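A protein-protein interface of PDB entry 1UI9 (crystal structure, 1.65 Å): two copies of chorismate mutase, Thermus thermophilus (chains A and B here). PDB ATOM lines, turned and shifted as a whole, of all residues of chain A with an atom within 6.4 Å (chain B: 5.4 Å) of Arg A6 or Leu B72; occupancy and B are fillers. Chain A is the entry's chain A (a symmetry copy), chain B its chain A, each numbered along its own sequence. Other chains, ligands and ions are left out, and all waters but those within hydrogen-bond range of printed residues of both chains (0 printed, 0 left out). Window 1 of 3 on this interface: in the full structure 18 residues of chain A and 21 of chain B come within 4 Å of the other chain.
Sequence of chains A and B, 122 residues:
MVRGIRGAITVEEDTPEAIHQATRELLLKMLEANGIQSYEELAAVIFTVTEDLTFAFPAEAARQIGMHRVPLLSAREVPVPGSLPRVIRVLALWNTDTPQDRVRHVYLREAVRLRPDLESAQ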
ATOM      1  N   GLY A   4      27.087  22.307  11.150  1.00  0.00           N
ATOM      2  CA  GLY A   4      28.047  21.334  10.673  1.00  0.00           C
ATOM      3  C   GLY A   4      28.384  21.631   9.222  1.00  0.00           C
ATOM      4  O   GLY A   4      27.542  22.120   8.462  1.00  0.00           O
ATOM      5  N   ILE A   5      29.624  21.364   8.837  1.00  0.00           N
ATOM      6  CA  ILE A   5      30.048  21.563   7.459  1.00  0.00           C
ATOM      7  C   ILE A   5      30.536  20.205   6.982  1.00  0.00           C
ATOM      8  O   ILE A   5      31.344  19.564   7.650  1.00  0.00           O
ATOM      9  CB  ILE A   5      31.236  22.546   7.319  1.00  0.00           C
ATOM     10  CG1 ILE A   5      30.967  23.849   8.079  1.00  0.00           C
ATOM     11  CG2 ILE A   5      31.448  22.861   5.842  1.00  0.00           C
ATOM     12  CD1 ILE A   5      32.124  24.830   8.001  1.00  0.00           C
ATOM     13  N   ARG A   6      30.044  19.757   5.838  1.00  0.00           N
ATOM     14  CA  ARG A   6      30.478  18.471   5.316  1.00  0.00           C
ATOM     15  C   ARG A   6      31.467  18.650   4.181  1.00  0.00           C
ATOM     16  O   ARG A   6      31.414  19.632   3.433  1.00  0.00           O
ATOM     17  CB  ARG A   6      29.286  17.642   4.825  1.00  0.00           C
ATOM     18  CG  ARG A   6      28.584  16.817   5.911  1.00  0.00           C
ATOM     19  CD  ARG A   6      29.552  15.838   6.592  1.00  0.00           C
ATOM     20  NE  ARG A   6      30.440  15.184   5.631  1.00  0.00           N
ATOM     21  CZ  ARG A   6      30.066  14.244   4.772  1.00  0.00           C
ATOM     22  NH1 ARG A   6      28.811  13.815   4.750  1.00  0.00           N
ATOM     23  NH2 ARG A   6      30.941  13.761   3.899  1.00  0.00           N
ATOM     24  N   GLY A   7      32.381  17.697   4.079  1.00  0.00           N
ATOM     25  CA  GLY A   7      33.368  17.709   3.022  1.00  0.00           C
ATOM     26  C   GLY A   7      33.673  16.273   2.653  1.00  0.00           C
ATOM     27  O   GLY A   7      33.478  15.360   3.459  1.00  0.00           O
ATOM     28  N   ALA A   8      34.120  16.061   1.423  1.00  0.00           N
ATOM     29  CA  ALA A   8      34.483  14.728   0.969  1.00  0.00           C
ATOM     30  C   ALA A   8      35.429  14.873  -0.207  1.00  0.00           C
ATOM     31  O   ALA A   8      35.280  15.785  -1.032  1.00  0.00           O
ATOM     32  CB  ALA A   8      33.245  13.933   0.560  1.00  0.00           C
ATOM     33  N   LEU A  26      41.007  19.469   0.955  1.00  0.00           N
ATOM     34  CA  LEU A  26      39.604  19.519   1.348  1.00  0.00           C
ATOM     35  C   LEU A  26      39.370  20.488   2.499  1.00  0.00           C
ATOM     36  O   LEU A  26      38.450  21.308   2.449  1.00  0.00           O
ATOM     37  CB  LEU A  26      39.112  18.124   1.739  1.00  0.00           C
ATOM     38  CG  LEU A  26      37.678  18.055   2.272  1.00  0.00           C
ATOM     39  CD1 LEU A  26      36.696  18.525   1.203  1.00  0.00           C
ATOM     40  CD2 LEU A  26      37.366  16.620   2.686  1.00  0.00           C
ATOM     41  N   MET A  30      37.048  23.858   2.343  1.00  0.00           N
ATOM     42  CA  MET A  30      35.863  23.955   3.194  1.00  0.00           C
ATOM     43  C   MET A  30      35.903  25.283   3.948  1.00  0.00           C
ATOM     44  O   MET A  30      34.876  25.940   4.141  1.00  0.00           O
ATOM     45  CB  MET A  30      35.829  22.800   4.204  1.00  0.00           C
ATOM     46  CG  MET A  30      35.464  21.457   3.604  1.00  0.00           C
ATOM     47  SD  MET A  30      35.630  20.127   4.819  1.00  0.00           S
ATOM     48  CE  MET A  30      34.183  20.427   5.843  1.00  0.00           C
ATOM     49  N   THR A  48      36.094  10.734   8.710  1.00  0.00           N
ATOM     50  CA  THR A  48      35.796   9.311   8.570  1.00  0.00           C
ATOM     51  C   THR A  48      36.672   8.902   7.393  1.00  0.00           C
ATOM     52  O   THR A  48      36.906   9.691   6.463  1.00  0.00           O
ATOM     53  CB  THR A  48      34.308   8.940   8.283  1.00  0.00           C
ATOM     54  OG1 THR A  48      33.954   9.288   6.943  1.00  0.00           O
ATOM     55  CG2 THR A  48      33.383   9.618   9.280  1.00  0.00           C
ATOM     56  N   ILE A  88      37.841  10.354   1.984  1.00  0.00           N
ATOM     57  CA  ILE A  88      38.126  10.984   3.260  1.00  0.00           C
ATOM     58  C   ILE A  88      36.970  11.953   3.413  1.00  0.00           C
ATOM     59  O   ILE A  88      36.751  12.803   2.543  1.00  0.00           O
ATOM     60  CB  ILE A  88      39.447  11.783   3.247  1.00  0.00           C
ATOM     61  CG1 ILE A  88      40.636  10.825   3.134  1.00  0.00           C
ATOM     62  CG2 ILE A  88      39.577  12.606   4.535  1.00  0.00           C
ATOM     63  CD1 ILE A  88      40.770   9.865   4.317  1.00  0.00           C
ATOM     64  N   ARG A  89      36.211  11.807   4.493  1.00  0.00           N
ATOM     65  CA  ARG A  89      35.080  12.699   4.738  1.00  0.00           C
ATOM     66  C   ARG A  89      35.336  13.549   5.967  1.00  0.00           C
ATOM     67  O   ARG A  89      36.028  13.131   6.893  1.00  0.00           O
ATOM     68  CB  ARG A  89      33.794  11.899   4.934  1.00  0.00           C
ATOM     69  CG  ARG A  89      33.266  11.228   3.665  1.00  0.00           C
ATOM     70  CD  ARG A  89      31.989  10.457   3.968  1.00  0.00           C
ATOM     71  NE  ARG A  89      31.316   9.922   2.781  1.00  0.00           N
ATOM     72  CZ  ARG A  89      31.652   8.798   2.150  1.00  0.00           C
ATOM     73  NH1 ARG A  89      32.670   8.061   2.570  1.00  0.00           N
ATOM     74  NH2 ARG A  89      30.947   8.389   1.102  1.00  0.00           N
ATOM     75  N   VAL A  90      34.773  14.751   5.968  1.00  0.00           N
ATOM     76  CA  VAL A  90      34.939  15.661   7.087  1.00  0.00           C
ATOM     77  C   VAL A  90      33.609  16.231   7.564  1.00  0.00           C
ATOM     78  O   VAL A  90      32.715  16.493   6.759  1.00  0.00           O
ATOM     79  CB  VAL A  90      35.834  16.864   6.705  1.00  0.00           C
ATOM     80  CG1 VAL A  90      35.923  17.841   7.871  1.00  0.00           C
ATOM     81  CG2 VAL A  90      37.218  16.382   6.303  1.00  0.00           C
ATOM     82  N   LEU A  91      33.485  16.394   8.878  1.00  0.00           N
ATOM     83  CA  LEU A  91      32.316  17.029   9.484  1.00  0.00           C
ATOM     84  C   LEU A  91      32.893  18.042  10.461  1.00  0.00           C
ATOM     85  O   LEU A  91      33.344  17.685  11.547  1.00  0.00           O
ATOM     86  CB  LEU A  91      31.419  16.046  10.248  1.00  0.00           C
ATOM     87  CG  LEU A  91      30.331  16.756  11.080  1.00  0.00           C
ATOM     88  CD1 LEU A  91      29.412  17.562  10.157  1.00  0.00           C
ATOM     89  CD2 LEU A  91      29.527  15.740  11.878  1.00  0.00           C
ATOM     90  N   ALA A  92      32.905  19.308  10.058  1.00  0.00           N
ATOM     91  CA  ALA A  92      33.425  20.368  10.902  1.00  0.00           C
ATOM     92  C   ALA A  92      32.266  21.016  11.650  1.00  0.00           C
ATOM     93  O   ALA A  92      31.267  21.391  11.038  1.00  0.00           O
ATOM     94  CB  ALA A  92      34.146  21.404  10.040  1.00  0.00           C
ATOM     95  N   VAL A 103      25.320  27.469   4.482  1.00  0.00           N
ATOM     96  CA  VAL A 103      26.573  26.768   4.741  1.00  0.00           C
ATOM     97  C   VAL A 103      26.992  26.077   3.446  1.00  0.00           C
ATOM     98  O   VAL A 103      26.170  25.457   2.778  1.00  0.00           O
ATOM     99  CB  VAL A 103      26.401  25.698   5.849  1.00  0.00           C
ATOM    100  CG1 VAL A 103      27.680  24.887   5.995  1.00  0.00           C
ATOM    101  CG2 VAL A 103      26.051  26.368   7.168  1.00  0.00           C
ATOM    102  N   ARG A 104      28.269  26.190   3.092  1.00  0.00           N
ATOM    103  CA  ARG A 104      28.768  25.572   1.873  1.00  0.00           C
ATOM    104  C   ARG A 104      29.477  24.253   2.147  1.00  0.00           C
ATOM    105  O   ARG A 104      30.480  24.218   2.853  1.00  0.00           O
ATOM    106  CB  ARG A 104      29.720  26.524   1.143  1.00  0.00           C
ATOM    107  CG  ARG A 104      29.066  27.841   0.743  1.00  0.00           C
ATOM    108  CD  ARG A 104      27.712  27.583   0.103  1.00  0.00           C
ATOM    109  NE  ARG A 104      26.930  28.804  -0.073  1.00  0.00           N
ATOM    110  CZ  ARG A 104      25.600  28.833  -0.130  1.00  0.00           C
ATOM    111  NH1 ARG A 104      24.905  27.706  -0.019  1.00  0.00           N
ATOM    112  NH2 ARG A 104      24.965  29.986  -0.300  1.00  0.00           N
ATOM    113  N   HIS A 105      28.940  23.176   1.583  1.00  0.00           N
ATOM    114  CA  HIS A 105      29.512  21.843   1.744  1.00  0.00           C
ATOM    115  C   HIS A 105      30.368  21.567   0.520  1.00  0.00           C
ATOM    116  O   HIS A 105      29.977  21.875  -0.607  1.00  0.00           O
ATOM    117  CB  HIS A 105      28.383  20.831   1.900  1.00  0.00           C
ATOM    118  CG  HIS A 105      27.464  21.163   3.030  1.00  0.00           C
ATOM    119  ND1 HIS A 105      27.833  21.018   4.350  1.00  0.00           N
ATOM    120  CD2 HIS A 105      26.239  21.742   3.042  1.00  0.00           C
ATOM    121  CE1 HIS A 105      26.878  21.496   5.128  1.00  0.00           C
ATOM    122  NE2 HIS A 105      25.899  21.943   4.358  1.00  0.00           N
ATOM    123  N   VAL A 106      31.536  20.977   0.746  1.00  0.00           N
ATOM    124  CA  VAL A 106      32.492  20.747  -0.327  1.00  0.00           C
ATOM    125  C   VAL A 106      32.775  19.301  -0.724  1.00  0.00           C
ATOM    126  O   VAL A 106      33.218  18.493   0.092  1.00  0.00           O
ATOM    127  CB  VAL A 106      33.818  21.435   0.036  1.00  0.00           C
ATOM    128  CG1 VAL A 106      34.867  21.171  -1.024  1.00  0.00           C
ATOM    129  CG2 VAL A 106      33.581  22.931   0.220  1.00  0.00           C
ATOM    130  N   TYR A 107      32.520  18.997  -1.994  1.00  0.00           N
ATOM    131  CA  TYR A 107      32.750  17.667  -2.547  1.00  0.00           C
ATOM    132  C   TYR A 107      33.724  17.797  -3.711  1.00  0.00           C
ATOM    133  O   TYR A 107      33.427  18.455  -4.715  1.00  0.00           O
ATOM    134  CB  TYR A 107      31.422  17.054  -2.992  1.00  0.00           C
ATOM    135  CG  TYR A 107      30.600  16.576  -1.818  1.00  0.00           C
ATOM    136  CD1 TYR A 107      30.503  15.218  -1.524  1.00  0.00           C
ATOM    137  CD2 TYR A 107      29.991  17.487  -0.951  1.00  0.00           C
ATOM    138  CE1 TYR A 107      29.828  14.773  -0.393  1.00  0.00           C
ATOM    139  CE2 TYR A 107      29.312  17.051   0.190  1.00  0.00           C
ATOM    140  CZ  TYR A 107      29.240  15.691   0.459  1.00  0.00           C
ATOM    141  OH  TYR A 107      28.597  15.238   1.589  1.00  0.00           O
ATOM    142  N   LEU A 114      28.979  11.676  -4.996  1.00  0.00           N
ATOM    143  CA  LEU A 114      28.241  11.388  -3.771  1.00  0.00           C
ATOM    144  C   LEU A 114      26.967  12.219  -3.649  1.00  0.00           C
ATOM    145  O   LEU A 114      25.983  11.769  -3.063  1.00  0.00           O
ATOM    146  CB  LEU A 114      29.136  11.622  -2.548  1.00  0.00           C
ATOM    147  CG  LEU A 114      30.378  10.729  -2.453  1.00  0.00           C
ATOM    148  CD1 LEU A 114      31.233  11.160  -1.266  1.00  0.00           C
ATOM    149  CD2 LEU A 114      29.960   9.272  -2.309  1.00  0.00           C
ATOM    150  N   VAL B  45      23.885  15.489  12.259  1.00  0.00           N
ATOM    151  CA  VAL B  45      23.401  14.198  12.723  1.00  0.00           C
ATOM    152  C   VAL B  45      24.451  13.145  12.401  1.00  0.00           C
ATOM    153  O   VAL B  45      24.925  13.051  11.271  1.00  0.00           O
ATOM    154  CB  VAL B  45      22.086  13.797  12.041  1.00  0.00           C
ATOM    155  CG1 VAL B  45      21.687  12.391  12.468  1.00  0.00           C
ATOM    156  CG2 VAL B  45      20.994  14.793  12.393  1.00  0.00           C
ATOM    157  N   PHE B  47      25.419   9.014  12.598  1.00  0.00           N
ATOM    158  CA  PHE B  47      24.856   7.670  12.712  1.00  0.00           C
ATOM    159  C   PHE B  47      25.978   6.672  12.973  1.00  0.00           C
ATOM    160  O   PHE B  47      27.119   6.911  12.583  1.00  0.00           O
ATOM    161  CB  PHE B  47      24.227   7.206  11.388  1.00  0.00           C
ATOM    162  CG  PHE B  47      23.116   8.067  10.875  1.00  0.00           C
ATOM    163  CD1 PHE B  47      21.805   7.857  11.293  1.00  0.00           C
ATOM    164  CD2 PHE B  47      23.367   9.052   9.926  1.00  0.00           C
ATOM    165  CE1 PHE B  47      20.764   8.613  10.769  1.00  0.00           C
ATOM    166  CE2 PHE B  47      22.328   9.815   9.394  1.00  0.00           C
ATOM    167  CZ  PHE B  47      21.019   9.590   9.821  1.00  0.00           C
ATOM    168  N   ALA B  59      21.638   7.731   5.489  1.00  0.00           N
ATOM    169  CA  ALA B  59      21.571   9.077   4.937  1.00  0.00           C
ATOM    170  C   ALA B  59      20.418   9.242   3.951  1.00  0.00           C
ATOM    171  O   ALA B  59      19.812  10.314   3.873  1.00  0.00           O
ATOM    172  CB  ALA B  59      22.884   9.427   4.264  1.00  0.00           C
ATOM    173  N   ALA B  62      17.207  10.007   5.748  1.00  0.00           N
ATOM    174  CA  ALA B  62      17.150  11.393   6.186  1.00  0.00           C
ATOM    175  C   ALA B  62      16.785  12.275   4.995  1.00  0.00           C
ATOM    176  O   ALA B  62      16.021  13.229   5.124  1.00  0.00           O
ATOM    177  CB  ALA B  62      18.500  11.816   6.768  1.00  0.00           C
ATOM    178  N   ARG B  63      17.339  11.945   3.833  1.00  0.00           N
ATOM    179  CA  ARG B  63      17.071  12.698   2.617  1.00  0.00           C
ATOM    180  C   ARG B  63      15.610  12.577   2.206  1.00  0.00           C
ATOM    181  O   ARG B  63      14.990  13.559   1.800  1.00  0.00           O
ATOM    182  CB  ARG B  63      17.970  12.204   1.481  1.00  0.00           C
ATOM    183  CG  ARG B  63      17.476  12.562   0.088  1.00  0.00           C
ATOM    184  CD  ARG B  63      18.528  12.266  -0.965  1.00  0.00           C
ATOM    185  NE  ARG B  63      19.601  13.255  -0.940  1.00  0.00           N
ATOM    186  CZ  ARG B  63      20.895  12.959  -0.987  1.00  0.00           C
ATOM    187  NH1 ARG B  63      21.287  11.693  -1.056  1.00  0.00           N
ATOM    188  NH2 ARG B  63      21.796  13.931  -0.969  1.00  0.00           N
ATOM    189  N   MET B  67      15.818  16.071   4.931  1.00  0.00           N
ATOM    190  CA  MET B  67      16.978  16.590   5.649  1.00  0.00           C
ATOM    191  C   MET B  67      18.176  16.809   4.721  1.00  0.00           C
ATOM    192  O   MET B  67      19.323  16.593   5.106  1.00  0.00           O
ATOM    193  CB  MET B  67      17.364  15.640   6.782  1.00  0.00           C
ATOM    194  CG  MET B  67      16.262  15.427   7.807  1.00  0.00           C
ATOM    195  SD  MET B  67      16.770  14.294   9.109  1.00  0.00           S
ATOM    196  CE  MET B  67      17.978  15.267   9.963  1.00  0.00           C
ATOM    197  N   VAL B  70      20.843  19.066   6.189  1.00  0.00           N
ATOM    198  CA  VAL B  70      21.389  18.701   7.496  1.00  0.00           C
ATOM    199  C   VAL B  70      22.655  17.876   7.276  1.00  0.00           C
ATOM    200  O   VAL B  70      22.611  16.830   6.633  1.00  0.00           O
ATOM    201  CB  VAL B  70      20.390  17.850   8.308  1.00  0.00           C
ATOM    202  CG1 VAL B  70      20.949  17.574   9.701  1.00  0.00           C
ATOM    203  CG2 VAL B  70      19.054  18.569   8.404  1.00  0.00           C
ATOM    204  N   PRO B  71      23.803  18.343   7.791  1.00  0.00           N
ATOM    205  CA  PRO B  71      25.039  17.575   7.599  1.00  0.00           C
ATOM    206  C   PRO B  71      24.980  16.232   8.324  1.00  0.00           C
ATOM    207  O   PRO B  71      24.649  16.161   9.511  1.00  0.00           O
ATOM    208  CB  PRO B  71      26.121  18.513   8.137  1.00  0.00           C
ATOM    209  CG  PRO B  71      25.403  19.339   9.141  1.00  0.00           C
ATOM    210  CD  PRO B  71      24.064  19.608   8.498  1.00  0.00           C
ATOM    211  N   LEU B  72      25.302  15.171   7.592  1.00  0.00           N
ATOM    212  CA  LEU B  72      25.250  13.824   8.138  1.00  0.00           C
ATOM    213  C   LEU B  72      26.584  13.097   8.031  1.00  0.00           C
ATOM    214  O   LEU B  72      27.358  13.321   7.096  1.00  0.00           O
ATOM    215  CB  LEU B  72      24.191  13.012   7.393  1.00  0.00           C
ATOM    216  CG  LEU B  72      22.828  13.665   7.153  1.00  0.00           C
ATOM    217  CD1 LEU B  72      22.013  12.801   6.205  1.00  0.00           C
ATOM    218  CD2 LEU B  72      22.099  13.855   8.475  1.00  0.00           C
ATOM    219  N   LEU B  73      26.840  12.218   8.992  1.00  0.00           N
ATOM    220  CA  LEU B  73      28.056  11.420   8.997  1.00  0.00           C
ATOM    221  C   LEU B  73      27.709  10.039   9.559  1.00  0.00           C
ATOM    222  O   LEU B  73      26.914   9.926  10.497  1.00  0.00           O
ATOM    223  CB  LEU B  73      29.134  12.095   9.846  1.00  0.00           C
ATOM    224  CG  LEU B  73      30.576  11.651   9.574  1.00  0.00           C
ATOM    225  CD1 LEU B  73      30.974  12.016   8.139  1.00  0.00           C
ATOM    226  CD2 LEU B  73      31.505  12.319  10.567  1.00  0.00           C
ATOM    227  N   SER B  74      28.294   8.993   8.984  1.00  0.00           N
ATOM    228  CA  SER B  74      28.021   7.625   9.434  1.00  0.00           C
ATOM    229  C   SER B  74      29.306   6.849   9.704  1.00  0.00           C
ATOM    230  O   SER B  74      30.167   6.726   8.830  1.00  0.00           O
ATOM    231  CB  SER B  74      27.193   6.872   8.390  1.00  0.00           C
ATOM    232  OG  SER B  74      27.908   6.723   7.177  1.00  0.00           O
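NH1 of Arg A6 lies within hydrogen-bond range of O of Leu B72, 2.8 Å away.
N of Phe B47 sits at hydrogen-bond distance from O of Leu B73 (2.7 Å).
The guanidinium group (NE) of Arg A6 lies within hydrogen-bond range of the backbone carbonyl oxygen (O) of Val A90 (2.9 Å).
N of Arg A89 lies within hydrogen-bond range of O of Thr A48 (3.0 Å).
O of Val B45 is in hydrogen-bond range of N of Leu B73, at 3.1 Å.
The guanidinium group (NH1) of Arg A6 lies within hydrogen-bond range of the side-chain hydroxyl (OH) of Tyr A107.
N of Val A106 lies within hydrogen-bond range of O of Arg A6, 3.0 Å away.
Gly A4 touches Pro B71.
Pro B71 touches Arg A6 (CB to CG, 3.7 Å).
Leu B73 touches Thr A48 (CG to CG2, 3.5 Å).
Leu A91 touches Pro B71 (CD1 to CB, 3.98 Å).
Leu A91 touches Leu B73.
Of chain B, only Pro B71 and Leu B72 come within 4 Å of Arg A6.
Leu B72 touches one residue of chain A.
Of the printed residues of chain B, Thr A48 touches Leu B73.
Printed residues of chain A within 4 Å of Leu B73: Thr A48 (3.5 Å) and Leu A91 (3.7 Å).
Printed residues of chain B within 4 Å of Leu A91: Pro B71 (3.98 Å) and Leu B73 (3.7 Å).
Printed residues of chain B within 4 Å of Gly A4: Pro B71.
Ala A92 touches none of the printed residues of chain B.
Leu A26 touches none of the printed residues of chain B.
The nearest residue of chain B that does not touch Arg A6 is Leu B73 (4.1 Å).
Hydrophobic or aromatic side chains of chain B within 4 Å of the printed part of chain A: Pro B71 and Leu B73.
Printed residues of chain A that touch a printed residue of chain B: Gly A4, Arg A6, Thr A48 and Leu A91.
Hydrophobic or aromatic side chains of chain A that line the printed part of chain B: Leu A91.
Among the printed residues, no Asp or Glu carboxylate lies within 4 Å of a Lys or Arg side-chain nitrogen of the other chain.
No position is printed for both chains.
Of the 6 pairs that touch across the chains among the printed residues, none has its exchanged pair printed and touching as well.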
